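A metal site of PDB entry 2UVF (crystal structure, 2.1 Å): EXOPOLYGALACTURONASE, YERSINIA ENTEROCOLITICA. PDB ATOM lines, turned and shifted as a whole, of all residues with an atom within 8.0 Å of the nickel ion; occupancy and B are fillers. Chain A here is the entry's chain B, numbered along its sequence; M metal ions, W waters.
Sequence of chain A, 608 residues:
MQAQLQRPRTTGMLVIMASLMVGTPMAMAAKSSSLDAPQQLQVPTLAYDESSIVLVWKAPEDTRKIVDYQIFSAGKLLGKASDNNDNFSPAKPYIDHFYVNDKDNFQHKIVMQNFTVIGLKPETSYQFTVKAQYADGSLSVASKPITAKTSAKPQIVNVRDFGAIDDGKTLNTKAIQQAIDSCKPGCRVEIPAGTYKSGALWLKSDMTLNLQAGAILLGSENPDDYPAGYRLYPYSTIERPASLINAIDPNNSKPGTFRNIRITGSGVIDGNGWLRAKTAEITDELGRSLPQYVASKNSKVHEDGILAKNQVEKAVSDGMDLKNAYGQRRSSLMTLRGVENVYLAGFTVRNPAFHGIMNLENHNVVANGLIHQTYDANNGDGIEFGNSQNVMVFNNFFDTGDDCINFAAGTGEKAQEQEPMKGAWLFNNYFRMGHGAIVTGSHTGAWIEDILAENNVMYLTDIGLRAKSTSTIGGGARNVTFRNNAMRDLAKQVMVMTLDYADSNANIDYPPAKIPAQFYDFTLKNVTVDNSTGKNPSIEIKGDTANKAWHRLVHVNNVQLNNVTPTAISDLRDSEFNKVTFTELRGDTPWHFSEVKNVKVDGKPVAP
Along chain A the residues within 4 Å of the nickel ion span positions 376 to 435.
The side-chain hydroxyl of Thr 374 sits at hydrogen-bond distance from the backbone NH of Gly 401 (3.2 Å). The backbone NH (N) of Gly 401 is in hydrogen-bond range of the backbone carbonyl oxygen (O) of Gly 380 (3.1 Å). The backbone carbonyl oxygen (O) of Asp 402 lies within hydrogen-bond range of the backbone NH (N) of His 435 (2.9 Å).
The nickel ion is bound by water W1, at 2.0 Å. The backbone carbonyl oxygen (O) of Gly 401 binds the nickel ion (2.1 Å). OD2 of Asp 376 binds the nickel ion. The nickel ion is bound by water W2 (2.2 Å). NE2 of His 435 binds the nickel ion, at 2.3 Å. The nickel ion has five donor atoms within binding distance.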
ATOM      1  N   ALA A 295     -12.006  21.712  -4.961  1.00  0.00           N
ATOM      2  CA  ALA A 295     -12.335  22.584  -3.832  1.00  0.00           C
ATOM      3  C   ALA A 295     -12.990  23.859  -4.367  1.00  0.00           C
ATOM      4  O   ALA A 295     -12.317  24.682  -4.972  1.00  0.00           O
ATOM      5  CB  ALA A 295     -11.074  22.910  -3.037  1.00  0.00           C
ATOM      6  N   THR A 374     -12.934  12.182   0.634  1.00  0.00           N
ATOM      7  CA  THR A 374     -13.778  13.288   0.181  1.00  0.00           C
ATOM      8  C   THR A 374     -13.036  14.607   0.064  1.00  0.00           C
ATOM      9  O   THR A 374     -13.639  15.673  -0.011  1.00  0.00           O
ATOM     10  CB  THR A 374     -15.016  13.457   1.093  1.00  0.00           C
ATOM     11  OG1 THR A 374     -14.625  13.959   2.384  1.00  0.00           O
ATOM     12  CG2 THR A 374     -15.752  12.103   1.258  1.00  0.00           C
ATOM     13  N   TYR A 375     -11.703  14.540   0.038  1.00  0.00           N
ATOM     14  CA  TYR A 375     -10.882  15.755  -0.071  1.00  0.00           C
ATOM     15  C   TYR A 375     -10.949  16.118  -1.544  1.00  0.00           C
ATOM     16  O   TYR A 375     -10.740  15.235  -2.370  1.00  0.00           O
ATOM     17  CB  TYR A 375      -9.446  15.420   0.312  1.00  0.00           C
ATOM     18  CG  TYR A 375      -8.524  16.562   0.112  1.00  0.00           C
ATOM     19  CD1 TYR A 375      -8.368  17.499   1.118  1.00  0.00           C
ATOM     20  CD2 TYR A 375      -7.840  16.761  -1.110  1.00  0.00           C
ATOM     21  CE1 TYR A 375      -7.568  18.584   0.965  1.00  0.00           C
ATOM     22  CE2 TYR A 375      -7.021  17.867  -1.278  1.00  0.00           C
ATOM     23  CZ  TYR A 375      -6.875  18.760  -0.212  1.00  0.00           C
ATOM     24  OH  TYR A 375      -6.095  19.856  -0.294  1.00  0.00           O
ATOM     25  N   ASP A 376     -11.251  17.391  -1.898  1.00  0.00           N
ATOM     26  CA  ASP A 376     -11.476  18.499  -0.974  1.00  0.00           C
ATOM     27  C   ASP A 376     -12.843  19.115  -1.255  1.00  0.00           C
ATOM     28  O   ASP A 376     -12.977  20.333  -1.512  1.00  0.00           O
ATOM     29  CB  ASP A 376     -10.360  19.540  -1.171  1.00  0.00           C
ATOM     30  CG  ASP A 376     -10.254  20.515  -0.038  1.00  0.00           C
ATOM     31  OD1 ASP A 376      -9.453  21.474  -0.155  1.00  0.00           O
ATOM     32  OD2 ASP A 376     -10.949  20.326   1.008  1.00  0.00           O
ATOM     33  N   ALA A 377     -13.873  18.264  -1.183  1.00  0.00           N
ATOM     34  CA  ALA A 377     -15.278  18.655  -1.241  1.00  0.00           C
ATOM     35  C   ALA A 377     -15.669  19.642  -0.122  1.00  0.00           C
ATOM     36  O   ALA A 377     -15.558  19.304   1.068  1.00  0.00           O
ATOM     37  CB  ALA A 377     -16.177  17.379  -1.188  1.00  0.00           C
ATOM     38  N   ASN A 378     -16.137  20.847  -0.518  1.00  0.00           N
ATOM     39  CA  ASN A 378     -16.396  21.934   0.412  1.00  0.00           C
ATOM     40  C   ASN A 378     -17.551  21.560   1.361  1.00  0.00           C
ATOM     41  O   ASN A 378     -18.621  21.165   0.890  1.00  0.00           O
ATOM     42  CB  ASN A 378     -16.692  23.215  -0.374  1.00  0.00           C
ATOM     43  CG  ASN A 378     -16.685  24.486   0.477  1.00  0.00           C
ATOM     44  OD1 ASN A 378     -15.953  24.623   1.463  1.00  0.00           O
ATOM     45  ND2 ASN A 378     -17.477  25.407   0.081  1.00  0.00           N
ATOM     46  N   ASN A 379     -17.273  21.654   2.669  1.00  0.00           N
ATOM     47  CA  ASN A 379     -18.181  21.224   3.753  1.00  0.00           C
ATOM     48  C   ASN A 379     -18.299  19.720   3.865  1.00  0.00           C
ATOM     49  O   ASN A 379     -19.155  19.182   4.571  1.00  0.00           O
ATOM     50  CB  ASN A 379     -19.546  21.924   3.660  1.00  0.00           C
ATOM     51  CG  ASN A 379     -19.401  23.423   3.549  1.00  0.00           C
ATOM     52  OD1 ASN A 379     -19.704  24.014   2.508  1.00  0.00           O
ATOM     53  ND2 ASN A 379     -18.816  24.043   4.594  1.00  0.00           N
ATOM     54  N   GLY A 380     -17.380  19.037   3.195  1.00  0.00           N
ATOM     55  CA  GLY A 380     -17.398  17.584   3.169  1.00  0.00           C
ATOM     56  C   GLY A 380     -16.720  17.030   4.393  1.00  0.00           C
ATOM     57  O   GLY A 380     -15.679  16.393   4.270  1.00  0.00           O
ATOM     58  N   ASP A 381     -17.305  17.276   5.580  1.00  0.00           N
ATOM     59  CA  ASP A 381     -16.763  16.695   6.814  1.00  0.00           C
ATOM     60  C   ASP A 381     -17.029  15.202   6.857  1.00  0.00           C
ATOM     61  O   ASP A 381     -17.953  14.738   6.222  1.00  0.00           O
ATOM     62  CB  ASP A 381     -17.250  17.387   8.110  1.00  0.00           C
ATOM     63  CG  ASP A 381     -18.672  17.830   8.072  1.00  0.00           C
ATOM     64  OD1 ASP A 381     -19.470  17.243   7.304  1.00  0.00           O
ATOM     65  OD2 ASP A 381     -18.995  18.785   8.837  1.00  0.00           O
ATOM     66  N   THR A 400     -10.567  14.069   4.323  1.00  0.00           N
ATOM     67  CA  THR A 400     -11.872  14.744   4.212  1.00  0.00           C
ATOM     68  C   THR A 400     -11.782  16.143   3.613  1.00  0.00           C
ATOM     69  O   THR A 400     -10.754  16.831   3.717  1.00  0.00           O
ATOM     70  CB  THR A 400     -12.685  14.691   5.562  1.00  0.00           C
ATOM     71  OG1 THR A 400     -11.885  15.167   6.639  1.00  0.00           O
ATOM     72  CG2 THR A 400     -13.106  13.262   5.915  1.00  0.00           C
ATOM     73  N   GLY A 401     -12.887  16.591   3.000  1.00  0.00           N
ATOM     74  CA  GLY A 401     -12.985  17.960   2.516  1.00  0.00           C
ATOM     75  C   GLY A 401     -13.034  19.020   3.606  1.00  0.00           C
ATOM     76  O   GLY A 401     -12.674  20.176   3.363  1.00  0.00           O
ATOM     77  N   ASP A 402     -13.459  18.647   4.803  1.00  0.00           N
ATOM     78  CA  ASP A 402     -13.639  19.608   5.878  1.00  0.00           C
ATOM     79  C   ASP A 402     -13.257  18.894   7.156  1.00  0.00           C
ATOM     80  O   ASP A 402     -12.325  18.102   7.162  1.00  0.00           O
ATOM     81  CB  ASP A 402     -15.088  20.160   5.870  1.00  0.00           C
ATOM     82  CG  ASP A 402     -15.217  21.498   6.589  1.00  0.00           C
ATOM     83  OD1 ASP A 402     -15.040  21.525   7.823  1.00  0.00           O
ATOM     84  OD2 ASP A 402     -15.476  22.526   5.936  1.00  0.00           O
ATOM     85  N   ASP A 403     -13.984  19.116   8.251  1.00  0.00           N
ATOM     86  CA  ASP A 403     -13.619  18.526   9.535  1.00  0.00           C
ATOM     87  C   ASP A 403     -13.687  17.008   9.463  1.00  0.00           C
ATOM     88  O   ASP A 403     -14.613  16.468   8.885  1.00  0.00           O
ATOM     89  CB  ASP A 403     -14.539  19.020  10.632  1.00  0.00           C
ATOM     90  CG  ASP A 403     -14.387  20.498  10.913  1.00  0.00           C
ATOM     91  OD1 ASP A 403     -13.243  21.020  10.884  1.00  0.00           O
ATOM     92  OD2 ASP A 403     -15.417  21.121  11.191  1.00  0.00           O
ATOM     93  N   MET A 433      -5.911  14.081   5.636  1.00  0.00           N
ATOM     94  CA  MET A 433      -6.182  15.493   5.344  1.00  0.00           C
ATOM     95  C   MET A 433      -7.580  15.897   5.732  1.00  0.00           C
ATOM     96  O   MET A 433      -8.531  15.221   5.356  1.00  0.00           O
ATOM     97  CB  MET A 433      -5.947  15.809   3.859  1.00  0.00           C
ATOM     98  CG  MET A 433      -4.460  15.971   3.473  1.00  0.00           C
ATOM     99  SD  MET A 433      -4.259  16.751   1.873  1.00  0.00           S
ATOM    100  CE  MET A 433      -4.271  18.480   2.394  1.00  0.00           C
ATOM    101  N   GLY A 434      -7.720  17.022   6.445  1.00  0.00           N
ATOM    102  CA  GLY A 434      -9.034  17.483   6.910  1.00  0.00           C
ATOM    103  C   GLY A 434      -8.864  18.707   7.784  1.00  0.00           C
ATOM    104  O   GLY A 434      -7.741  19.075   8.115  1.00  0.00           O
ATOM    105  N   HIS A 435      -9.948  19.349   8.163  1.00  0.00           N
ATOM    106  CA  HIS A 435      -9.816  20.655   8.827  1.00  0.00           C
ATOM    107  C   HIS A 435      -9.465  20.627  10.332  1.00  0.00           C
ATOM    108  O   HIS A 435      -9.120  21.645  10.916  1.00  0.00           O
ATOM    109  CB  HIS A 435     -11.041  21.488   8.568  1.00  0.00           C
ATOM    110  CG  HIS A 435     -11.193  21.928   7.155  1.00  0.00           C
ATOM    111  ND1 HIS A 435     -12.046  22.936   6.794  1.00  0.00           N
ATOM    112  CD2 HIS A 435     -10.588  21.511   6.022  1.00  0.00           C
ATOM    113  CE1 HIS A 435     -11.973  23.118   5.477  1.00  0.00           C
ATOM    114  NE2 HIS A 435     -11.103  22.255   4.989  1.00  0.00           N
ATOM    115  N   ASP A 462      -4.972  19.482   9.132  1.00  0.00           N
ATOM    116  CA  ASP A 462      -4.812  20.872   9.564  1.00  0.00           C
ATOM    117  C   ASP A 462      -4.519  21.007  11.047  1.00  0.00           C
ATOM    118  O   ASP A 462      -3.481  21.552  11.457  1.00  0.00           O
ATOM    119  CB  ASP A 462      -6.033  21.692   9.215  1.00  0.00           C
ATOM    120  CG  ASP A 462      -6.137  21.984   7.749  1.00  0.00           C
ATOM    121  OD1 ASP A 462      -5.391  21.368   6.938  1.00  0.00           O
ATOM    122  OD2 ASP A 462      -7.013  22.823   7.403  1.00  0.00           O
HETATM  123 NI    NI M   1     -10.853  21.155   2.959  1.00  0.00          NI
HETATM  124  O   HOH W   1     -12.020  22.658   2.263  1.00  0.00           O
HETATM  125  O   HOH W   2      -9.776  19.303   3.526  1.00  0.00           O
